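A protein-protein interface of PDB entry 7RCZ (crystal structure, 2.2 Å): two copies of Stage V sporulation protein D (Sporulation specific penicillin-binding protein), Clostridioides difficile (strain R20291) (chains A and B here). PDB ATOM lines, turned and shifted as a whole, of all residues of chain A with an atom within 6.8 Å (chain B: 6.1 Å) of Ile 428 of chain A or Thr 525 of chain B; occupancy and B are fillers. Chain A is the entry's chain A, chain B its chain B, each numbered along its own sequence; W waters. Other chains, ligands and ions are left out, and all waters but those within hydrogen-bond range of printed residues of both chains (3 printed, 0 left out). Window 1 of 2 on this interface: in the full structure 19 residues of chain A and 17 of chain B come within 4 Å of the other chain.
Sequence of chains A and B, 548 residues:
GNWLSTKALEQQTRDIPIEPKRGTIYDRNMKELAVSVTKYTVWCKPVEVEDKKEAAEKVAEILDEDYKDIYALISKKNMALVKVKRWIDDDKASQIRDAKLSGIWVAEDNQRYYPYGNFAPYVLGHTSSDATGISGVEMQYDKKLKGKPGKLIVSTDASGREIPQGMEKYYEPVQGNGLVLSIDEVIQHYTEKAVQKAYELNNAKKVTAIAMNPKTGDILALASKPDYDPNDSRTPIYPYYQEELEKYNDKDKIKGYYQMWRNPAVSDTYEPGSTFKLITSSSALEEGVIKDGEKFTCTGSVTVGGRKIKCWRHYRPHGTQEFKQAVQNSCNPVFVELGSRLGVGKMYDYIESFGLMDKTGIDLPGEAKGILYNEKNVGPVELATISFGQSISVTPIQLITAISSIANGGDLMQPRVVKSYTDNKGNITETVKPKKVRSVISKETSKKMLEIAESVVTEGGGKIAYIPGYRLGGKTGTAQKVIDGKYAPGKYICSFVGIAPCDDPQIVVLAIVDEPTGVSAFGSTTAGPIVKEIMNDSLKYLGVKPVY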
ATOM      1  N   TYR A  26     -23.954   7.637 -13.061  1.00  0.00           N
ATOM      2  CA  TYR A  26     -23.246   6.361 -12.846  1.00  0.00           C
ATOM      3  C   TYR A  26     -21.942   6.400 -13.652  1.00  0.00           C
ATOM      4  O   TYR A  26     -21.870   7.055 -14.724  1.00  0.00           O
ATOM      5  CB  TYR A  26     -24.100   5.163 -13.289  1.00  0.00           C
ATOM      6  CG  TYR A  26     -25.458   5.016 -12.640  1.00  0.00           C
ATOM      7  CD1 TYR A  26     -26.584   5.564 -13.227  1.00  0.00           C
ATOM      8  CD2 TYR A  26     -25.648   4.251 -11.502  1.00  0.00           C
ATOM      9  CE1 TYR A  26     -27.835   5.431 -12.662  1.00  0.00           C
ATOM     10  CE2 TYR A  26     -26.901   4.087 -10.935  1.00  0.00           C
ATOM     11  CZ  TYR A  26     -28.001   4.693 -11.505  1.00  0.00           C
ATOM     12  OH  TYR A  26     -29.260   4.559 -10.971  1.00  0.00           O
ATOM     13  N   MET A  30     -21.867   1.169 -13.472  1.00  0.00           N
ATOM     14  CA  MET A  30     -23.104   1.510 -12.724  1.00  0.00           C
ATOM     15  C   MET A  30     -22.793   1.712 -11.239  1.00  0.00           C
ATOM     16  O   MET A  30     -23.678   1.454 -10.475  1.00  0.00           O
ATOM     17  CB  MET A  30     -24.155   0.400 -12.841  1.00  0.00           C
ATOM     18  CG  MET A  30     -24.540   0.068 -14.254  1.00  0.00           C
ATOM     19  SD  MET A  30     -25.006   1.545 -15.168  1.00  0.00           S
ATOM     20  CE  MET A  30     -26.581   1.956 -14.425  1.00  0.00           C
ATOM     21  N   VAL A 180     -25.238   7.328 -17.592  1.00  0.00           N
ATOM     22  CA  VAL A 180     -24.069   6.417 -17.406  1.00  0.00           C
ATOM     23  C   VAL A 180     -22.902   7.064 -18.136  1.00  0.00           C
ATOM     24  O   VAL A 180     -23.046   7.282 -19.357  1.00  0.00           O
ATOM     25  CB  VAL A 180     -24.358   5.018 -17.952  1.00  0.00           C
ATOM     26  CG1 VAL A 180     -23.187   4.057 -17.728  1.00  0.00           C
ATOM     27  CG2 VAL A 180     -25.644   4.460 -17.370  1.00  0.00           C
ATOM     28  N   LYS A 419     -22.359   8.060 -22.063  1.00  0.00           N
ATOM     29  CA  LYS A 419     -22.479   6.884 -22.956  1.00  0.00           C
ATOM     30  C   LYS A 419     -23.941   6.408 -23.019  1.00  0.00           C
ATOM     31  O   LYS A 419     -24.334   5.927 -24.091  1.00  0.00           O
ATOM     32  CB  LYS A 419     -21.523   5.790 -22.487  1.00  0.00           C
ATOM     33  CG  LYS A 419     -21.384   4.626 -23.457  1.00  0.00           C
ATOM     34  CD  LYS A 419     -21.102   5.079 -24.893  1.00  0.00           C
ATOM     35  CE  LYS A 419     -20.437   4.024 -25.737  1.00  0.00           C
ATOM     36  NZ  LYS A 419     -20.109   4.571 -27.081  1.00  0.00           N
ATOM     37  N   SER A 420     -24.720   6.526 -21.930  1.00  0.00           N
ATOM     38  CA  SER A 420     -26.091   5.950 -21.840  1.00  0.00           C
ATOM     39  C   SER A 420     -27.008   6.822 -20.962  1.00  0.00           C
ATOM     40  O   SER A 420     -26.520   7.594 -20.122  1.00  0.00           O
ATOM     41  CB  SER A 420     -26.050   4.527 -21.357  1.00  0.00           C
ATOM     42  OG  SER A 420     -25.175   3.686 -22.134  1.00  0.00           O
ATOM     43  N   TYR A 421     -28.305   6.753 -21.211  1.00  0.00           N
ATOM     44  CA  TYR A 421     -29.365   7.333 -20.357  1.00  0.00           C
ATOM     45  C   TYR A 421     -30.056   6.190 -19.623  1.00  0.00           C
ATOM     46  O   TYR A 421     -30.084   5.086 -20.186  1.00  0.00           O
ATOM     47  CB  TYR A 421     -30.357   8.135 -21.197  1.00  0.00           C
ATOM     48  CG  TYR A 421     -29.704   9.221 -22.007  1.00  0.00           C
ATOM     49  CD1 TYR A 421     -29.077   8.913 -23.193  1.00  0.00           C
ATOM     50  CD2 TYR A 421     -29.612  10.515 -21.540  1.00  0.00           C
ATOM     51  CE1 TYR A 421     -28.448   9.883 -23.950  1.00  0.00           C
ATOM     52  CE2 TYR A 421     -28.993  11.505 -22.281  1.00  0.00           C
ATOM     53  CZ  TYR A 421     -28.407  11.186 -23.492  1.00  0.00           C
ATOM     54  OH  TYR A 421     -27.756  12.108 -24.253  1.00  0.00           O
ATOM     55  N   THR A 422     -30.544   6.463 -18.409  1.00  0.00           N
ATOM     56  CA  THR A 422     -31.340   5.532 -17.571  1.00  0.00           C
ATOM     57  C   THR A 422     -32.709   6.157 -17.250  1.00  0.00           C
ATOM     58  O   THR A 422     -32.882   7.378 -17.379  1.00  0.00           O
ATOM     59  CB  THR A 422     -30.584   5.160 -16.289  1.00  0.00           C
ATOM     60  OG1 THR A 422     -30.632   6.288 -15.432  1.00  0.00           O
ATOM     61  CG2 THR A 422     -29.131   4.804 -16.498  1.00  0.00           C
ATOM     62  N   ASP A 423     -33.664   5.332 -16.853  1.00  0.00           N
ATOM     63  CA  ASP A 423     -34.889   5.782 -16.145  1.00  0.00           C
ATOM     64  C   ASP A 423     -34.453   6.151 -14.711  1.00  0.00           C
ATOM     65  O   ASP A 423     -33.215   6.183 -14.443  1.00  0.00           O
ATOM     66  CB  ASP A 423     -35.968   4.699 -16.277  1.00  0.00           C
ATOM     67  CG  ASP A 423     -35.629   3.374 -15.602  1.00  0.00           C
ATOM     68  OD1 ASP A 423     -34.575   3.291 -14.932  1.00  0.00           O
ATOM     69  OD2 ASP A 423     -36.410   2.418 -15.769  1.00  0.00           O
ATOM     70  N   GLY A 426     -32.553   2.972 -12.598  1.00  0.00           N
ATOM     71  CA  GLY A 426     -31.224   2.425 -12.947  1.00  0.00           C
ATOM     72  C   GLY A 426     -31.230   1.579 -14.216  1.00  0.00           C
ATOM     73  O   GLY A 426     -30.206   0.961 -14.519  1.00  0.00           O
ATOM     74  N   ASN A 427     -32.367   1.503 -14.912  1.00  0.00           N
ATOM     75  CA  ASN A 427     -32.519   0.758 -16.185  1.00  0.00           C
ATOM     76  C   ASN A 427     -31.996   1.634 -17.327  1.00  0.00           C
ATOM     77  O   ASN A 427     -32.459   2.761 -17.424  1.00  0.00           O
ATOM     78  CB  ASN A 427     -33.976   0.374 -16.472  1.00  0.00           C
ATOM     79  CG  ASN A 427     -34.616  -0.373 -15.320  1.00  0.00           C
ATOM     80  OD1 ASN A 427     -34.069  -1.377 -14.871  1.00  0.00           O
ATOM     81  ND2 ASN A 427     -35.763   0.101 -14.857  1.00  0.00           N
ATOM     82  N   ILE A 428     -31.092   1.106 -18.163  1.00  0.00           N
ATOM     83  CA  ILE A 428     -30.606   1.781 -19.397  1.00  0.00           C
ATOM     84  C   ILE A 428     -31.779   1.902 -20.357  1.00  0.00           C
ATOM     85  O   ILE A 428     -32.450   0.863 -20.593  1.00  0.00           O
ATOM     86  CB  ILE A 428     -29.493   0.989 -20.103  1.00  0.00           C
ATOM     87  CG1 ILE A 428     -28.375   0.525 -19.164  1.00  0.00           C
ATOM     88  CG2 ILE A 428     -28.980   1.798 -21.273  1.00  0.00           C
ATOM     89  CD1 ILE A 428     -27.580   1.632 -18.563  1.00  0.00           C
ATOM     90  N   THR A 429     -31.968   3.077 -20.954  1.00  0.00           N
ATOM     91  CA  THR A 429     -33.076   3.322 -21.903  1.00  0.00           C
ATOM     92  C   THR A 429     -32.512   3.493 -23.306  1.00  0.00           C
ATOM     93  O   THR A 429     -33.193   3.120 -24.250  1.00  0.00           O
ATOM     94  CB  THR A 429     -33.929   4.545 -21.542  1.00  0.00           C
ATOM     95  OG1 THR A 429     -33.038   5.641 -21.298  1.00  0.00           O
ATOM     96  CG2 THR A 429     -34.833   4.273 -20.356  1.00  0.00           C
ATOM     97  N   GLU A 430     -31.314   4.037 -23.413  1.00  0.00           N
ATOM     98  CA  GLU A 430     -30.713   4.462 -24.694  1.00  0.00           C
ATOM     99  C   GLU A 430     -29.199   4.482 -24.510  1.00  0.00           C
ATOM    100  O   GLU A 430     -28.752   4.851 -23.417  1.00  0.00           O
ATOM    101  CB  GLU A 430     -31.272   5.842 -25.045  1.00  0.00           C
ATOM    102  CG  GLU A 430     -30.513   6.523 -26.159  1.00  0.00           C
ATOM    103  CD  GLU A 430     -31.058   7.880 -26.566  1.00  0.00           C
ATOM    104  OE1 GLU A 430     -32.008   8.358 -25.909  1.00  0.00           O
ATOM    105  OE2 GLU A 430     -30.514   8.458 -27.534  1.00  0.00           O
ATOM    106  N   THR A 431     -28.438   4.055 -25.514  1.00  0.00           N
ATOM    107  CA  THR A 431     -26.971   4.167 -25.472  1.00  0.00           C
ATOM    108  C   THR A 431     -26.540   4.899 -26.751  1.00  0.00           C
ATOM    109  O   THR A 431     -27.171   4.676 -27.802  1.00  0.00           O
ATOM    110  CB  THR A 431     -26.345   2.801 -25.186  1.00  0.00           C
ATOM    111  OG1 THR A 431     -24.969   3.053 -24.906  1.00  0.00           O
ATOM    112  CG2 THR A 431     -26.485   1.817 -26.332  1.00  0.00           C
ATOM    113  N   LEU B 201     -18.504  -2.855 -32.526  1.00  0.00           N
ATOM    114  CA  LEU B 201     -18.836  -1.841 -31.491  1.00  0.00           C
ATOM    115  C   LEU B 201     -18.263  -2.245 -30.129  1.00  0.00           C
ATOM    116  O   LEU B 201     -17.806  -1.363 -29.427  1.00  0.00           O
ATOM    117  CB  LEU B 201     -20.355  -1.679 -31.430  1.00  0.00           C
ATOM    118  CG  LEU B 201     -20.859  -0.508 -30.592  1.00  0.00           C
ATOM    119  CD1 LEU B 201     -20.409   0.796 -31.196  1.00  0.00           C
ATOM    120  CD2 LEU B 201     -22.378  -0.513 -30.484  1.00  0.00           C
ATOM    121  N   ASN B 202     -18.229  -3.542 -29.815  1.00  0.00           N
ATOM    122  CA  ASN B 202     -17.936  -4.091 -28.474  1.00  0.00           C
ATOM    123  C   ASN B 202     -16.533  -4.682 -28.426  1.00  0.00           C
ATOM    124  O   ASN B 202     -16.160  -5.194 -27.333  1.00  0.00           O
ATOM    125  CB  ASN B 202     -18.953  -5.170 -28.099  1.00  0.00           C
ATOM    126  CG  ASN B 202     -20.321  -4.580 -27.852  1.00  0.00           C
ATOM    127  OD1 ASN B 202     -20.525  -3.908 -26.835  1.00  0.00           O
ATOM    128  ND2 ASN B 202     -21.220  -4.747 -28.813  1.00  0.00           N
ATOM    129  N   GLY B 460     -38.559  -2.600 -16.993  1.00  0.00           N
ATOM    130  CA  GLY B 460     -37.411  -3.085 -16.205  1.00  0.00           C
ATOM    131  C   GLY B 460     -36.116  -3.047 -16.987  1.00  0.00           C
ATOM    132  O   GLY B 460     -35.996  -2.190 -17.843  1.00  0.00           O
ATOM    133  N   GLY B 461     -35.214  -3.977 -16.673  1.00  0.00           N
ATOM    134  CA  GLY B 461     -33.803  -4.005 -17.099  1.00  0.00           C
ATOM    135  C   GLY B 461     -33.641  -4.240 -18.591  1.00  0.00           C
ATOM    136  O   GLY B 461     -32.516  -4.118 -19.048  1.00  0.00           O
ATOM    137  N   GLY B 462     -34.725  -4.566 -19.301  1.00  0.00           N
ATOM    138  CA  GLY B 462     -34.745  -4.860 -20.740  1.00  0.00           C
ATOM    139  C   GLY B 462     -35.219  -3.689 -21.574  1.00  0.00           C
ATOM    140  O   GLY B 462     -35.343  -3.884 -22.781  1.00  0.00           O
ATOM    141  N   LYS B 463     -35.492  -2.533 -20.956  1.00  0.00           N
ATOM    142  CA  LYS B 463     -36.034  -1.293 -21.594  1.00  0.00           C
ATOM    143  C   LYS B 463     -35.275  -0.903 -22.873  1.00  0.00           C
ATOM    144  O   LYS B 463     -35.905  -0.339 -23.756  1.00  0.00           O
ATOM    145  CB  LYS B 463     -35.953  -0.105 -20.622  1.00  0.00           C
ATOM    146  CG  LYS B 463     -37.260   0.246 -19.955  1.00  0.00           C
ATOM    147  CD  LYS B 463     -37.231   1.478 -19.061  1.00  0.00           C
ATOM    148  CE  LYS B 463     -38.246   1.339 -17.946  1.00  0.00           C
ATOM    149  NZ  LYS B 463     -38.725   2.645 -17.446  1.00  0.00           N
ATOM    150  N   ILE B 464     -33.960  -1.112 -22.939  1.00  0.00           N
ATOM    151  CA  ILE B 464     -33.131  -0.747 -24.131  1.00  0.00           C
ATOM    152  C   ILE B 464     -33.808  -1.309 -25.386  1.00  0.00           C
ATOM    153  O   ILE B 464     -33.727  -0.683 -26.441  1.00  0.00           O
ATOM    154  CB  ILE B 464     -31.680  -1.241 -23.979  1.00  0.00           C
ATOM    155  CG1 ILE B 464     -30.743  -0.671 -25.043  1.00  0.00           C
ATOM    156  CG2 ILE B 464     -31.608  -2.750 -23.965  1.00  0.00           C
ATOM    157  CD1 ILE B 464     -30.608   0.813 -25.002  1.00  0.00           C
ATOM    158  N   ALA B 465     -34.467  -2.455 -25.251  1.00  0.00           N
ATOM    159  CA  ALA B 465     -34.936  -3.258 -26.392  1.00  0.00           C
ATOM    160  C   ALA B 465     -36.380  -2.914 -26.721  1.00  0.00           C
ATOM    161  O   ALA B 465     -36.905  -3.486 -27.701  1.00  0.00           O
ATOM    162  CB  ALA B 465     -34.740  -4.725 -26.092  1.00  0.00           C
ATOM    163  N   SER B 520     -18.797  -0.744 -21.315  1.00  0.00           N
ATOM    164  CA  SER B 520     -19.652  -1.209 -20.208  1.00  0.00           C
ATOM    165  C   SER B 520     -20.159  -2.619 -20.557  1.00  0.00           C
ATOM    166  O   SER B 520     -20.778  -2.784 -21.627  1.00  0.00           O
ATOM    167  CB  SER B 520     -20.746  -0.181 -20.011  1.00  0.00           C
ATOM    168  OG  SER B 520     -21.649  -0.562 -19.016  1.00  0.00           O
ATOM    169  N   ALA B 521     -19.835  -3.604 -19.716  1.00  0.00           N
ATOM    170  CA  ALA B 521     -20.115  -5.043 -19.898  1.00  0.00           C
ATOM    171  C   ALA B 521     -21.451  -5.418 -19.248  1.00  0.00           C
ATOM    172  O   ALA B 521     -21.444  -6.146 -18.262  1.00  0.00           O
ATOM    173  CB  ALA B 521     -18.980  -5.851 -19.326  1.00  0.00           C
ATOM    174  N   PHE B 522     -22.572  -5.037 -19.846  1.00  0.00           N
ATOM    175  CA  PHE B 522     -23.917  -5.486 -19.382  1.00  0.00           C
ATOM    176  C   PHE B 522     -24.741  -6.042 -20.548  1.00  0.00           C
ATOM    177  O   PHE B 522     -24.597  -5.590 -21.697  1.00  0.00           O
ATOM    178  CB  PHE B 522     -24.633  -4.360 -18.635  1.00  0.00           C
ATOM    179  CG  PHE B 522     -23.930  -3.952 -17.364  1.00  0.00           C
ATOM    180  CD1 PHE B 522     -24.078  -4.698 -16.201  1.00  0.00           C
ATOM    181  CD2 PHE B 522     -23.105  -2.837 -17.326  1.00  0.00           C
ATOM    182  CE1 PHE B 522     -23.415  -4.346 -15.029  1.00  0.00           C
ATOM    183  CE2 PHE B 522     -22.445  -2.480 -16.155  1.00  0.00           C
ATOM    184  CZ  PHE B 522     -22.591  -3.241 -15.008  1.00  0.00           C
ATOM    185  N   GLY B 523     -25.583  -7.028 -20.249  1.00  0.00           N
ATOM    186  CA  GLY B 523     -26.544  -7.572 -21.222  1.00  0.00           C
ATOM    187  C   GLY B 523     -27.272  -6.461 -21.949  1.00  0.00           C
ATOM    188  O   GLY B 523     -27.364  -6.502 -23.192  1.00  0.00           O
ATOM    189  N   SER B 524     -27.806  -5.502 -21.202  1.00  0.00           N
ATOM    190  CA  SER B 524     -28.700  -4.467 -21.754  1.00  0.00           C
ATOM    191  C   SER B 524     -27.951  -3.679 -22.845  1.00  0.00           C
ATOM    192  O   SER B 524     -28.492  -3.582 -23.957  1.00  0.00           O
ATOM    193  CB  SER B 524     -29.225  -3.575 -20.673  1.00  0.00           C
ATOM    194  OG  SER B 524     -28.140  -2.945 -20.008  1.00  0.00           O
ATOM    195  N   THR B 525     -26.766  -3.131 -22.543  1.00  0.00           N
ATOM    196  CA  THR B 525     -26.043  -2.185 -23.435  1.00  0.00           C
ATOM    197  C   THR B 525     -25.350  -2.921 -24.598  1.00  0.00           C
ATOM    198  O   THR B 525     -25.285  -2.315 -25.675  1.00  0.00           O
ATOM    199  CB  THR B 525     -25.003  -1.352 -22.665  1.00  0.00           C
ATOM    200  OG1 THR B 525     -24.231  -2.225 -21.849  1.00  0.00           O
ATOM    201  CG2 THR B 525     -25.627  -0.318 -21.766  1.00  0.00           C
ATOM    202  N   THR B 526     -24.836  -4.138 -24.395  1.00  0.00           N
ATOM    203  CA  THR B 526     -24.042  -4.904 -25.404  1.00  0.00           C
ATOM    204  C   THR B 526     -24.967  -5.793 -26.246  1.00  0.00           C
ATOM    205  O   THR B 526     -24.863  -5.742 -27.470  1.00  0.00           O
ATOM    206  CB  THR B 526     -22.914  -5.729 -24.765  1.00  0.00           C
ATOM    207  OG1 THR B 526     -23.484  -6.789 -24.003  1.00  0.00           O
ATOM    208  CG2 THR B 526     -22.005  -4.935 -23.854  1.00  0.00           C
ATOM    209  N   ALA B 527     -25.825  -6.604 -25.626  1.00  0.00           N
ATOM    210  CA  ALA B 527     -26.664  -7.629 -26.299  1.00  0.00           C
ATOM    211  C   ALA B 527     -28.080  -7.097 -26.593  1.00  0.00           C
ATOM    212  O   ALA B 527     -28.714  -7.553 -27.581  1.00  0.00           O
ATOM    213  CB  ALA B 527     -26.661  -8.871 -25.455  1.00  0.00           C
ATOM    214  N   GLY B 528     -28.575  -6.152 -25.792  1.00  0.00           N
ATOM    215  CA  GLY B 528     -29.917  -5.564 -25.950  1.00  0.00           C
ATOM    216  C   GLY B 528     -30.114  -4.933 -27.325  1.00  0.00           C
ATOM    217  O   GLY B 528     -31.154  -5.144 -27.941  1.00  0.00           O
ATOM    218  N   PRO B 529     -29.173  -4.103 -27.849  1.00  0.00           N
ATOM    219  CA  PRO B 529     -29.341  -3.522 -29.186  1.00  0.00           C
ATOM    220  C   PRO B 529     -29.334  -4.560 -30.323  1.00  0.00           C
ATOM    221  O   PRO B 529     -29.901  -4.280 -31.359  1.00  0.00           O
ATOM    222  CB  PRO B 529     -28.177  -2.510 -29.332  1.00  0.00           C
ATOM    223  CG  PRO B 529     -27.754  -2.240 -27.902  1.00  0.00           C
ATOM    224  CD  PRO B 529     -27.998  -3.544 -27.150  1.00  0.00           C
HETATM  225  O   HOH W   1     -32.399  -1.781 -20.845  1.00  0.00           O
HETATM  226  O   HOH W   2     -30.628  -1.743 -17.861  1.00  0.00           O
HETATM  227  O   HOH W   3     -35.987   2.563 -24.507  1.00  0.00           O
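Along chain B the printed residues that touch a printed residue of chain A span positions 460 to 525.
Water W1 lies within hydrogen-bond range of the backbone carbonyl oxygen of Ile 428 of chain A (2.7 Å), the backbone NH of Ile 464 of chain B (2.7 Å), the backbone carbonyl oxygen of Gly 461 of chain B (3.0 Å) and the backbone NH of Lys 463 of chain B (3.2 Å). Water W3 bridges the backbone carbonyl oxygen of Thr 429 of chain A and the backbone carbonyl oxygen of Lys 463 of chain B. Water W2 lies within hydrogen-bond range of the backbone NH (N) of Ile 428 of chain A, the backbone carbonyl oxygen (O) of Gly 461 of chain B and the side-chain hydroxyl (OG) of Ser 524 of chain B.
Of the printed residues of chain B, Glu 430 of chain A touches Ile 464 (3.7 Å). Printed residues of chain A within 4 Å of Ile 464 of chain B: Ile 428 (3.4 Å), Thr 429 (3.5 Å), Glu 430 (3.7 Å) and Thr 431 (3.9 Å). The nearest residue of chain B that does not touch Ile 428 of chain A is Gly 461 of chain B (5.2 Å).
OG1 of Thr 431 of chain A lies within hydrogen-bond range of O of Lys 419 of chain A (3.1 Å). The side-chain hydroxyl (OG) of Ser 420 of chain A sits at hydrogen-bond distance from the side-chain hydroxyl (OG1) of Thr 431 of chain A (2.9 Å). The backbone NH of Thr 429 of chain A is in hydrogen-bond range of the backbone carbonyl oxygen of Tyr 421 of chain A (2.9 Å). N of Tyr 421 of chain A lies within hydrogen-bond range of O of Glu 430 of chain A, 2.9 Å away. OG1 of Thr 525 of chain B is in hydrogen-bond range of O of Phe 522 of chain B, at 3.4 Å. The side-chain hydroxyl (OG1) of Thr 526 of chain B sits at hydrogen-bond distance from the backbone carbonyl oxygen (O) of Phe 522 of chain B, at 2.8 Å.
The side-chain carboxylate (OD2) of Asp 423 of chain A lies within salt-bridge range of the side-chain amino group (NZ) of Lys 463 of chain B (2.9 Å). The backbone NH of Gly 461 of chain B lies within hydrogen-bond range of the side-chain amide oxygen of Asn 427 of chain A, at 3.4 Å. The backbone NH of Ile 464 of chain B lies within hydrogen-bond range of the backbone carbonyl oxygen of Ile 428 of chain A.
Phe 522 of chain B touches Met 30 of chain A. Gly 460 of chain B touches Asn 427 of chain A (C to OD1, 3.4 Å). O of Ile 428 of chain A touches CB of Lys 463 of chain B, 3.6 Å away. Ile 428 of chain A touches Ser 524 of chain B. Ile 428 of chain A touches Thr 525 of chain B (CG1 to CG2, 3.9 Å). Thr 429 of chain A touches Lys 463 of chain B (CG2 to CD, 3.9 Å). Thr 429 of chain A touches Ile 464 of chain B. N of Glu 430 of chain A touches CD1 of Ile 464 of chain B, 3.7 Å away. Thr 431 of chain A touches Ile 464 of chain B.
No position is printed for both chains. Of the 12 pairs that touch across the chains among the printed residues, none has its exchanged pair printed and touching as well.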
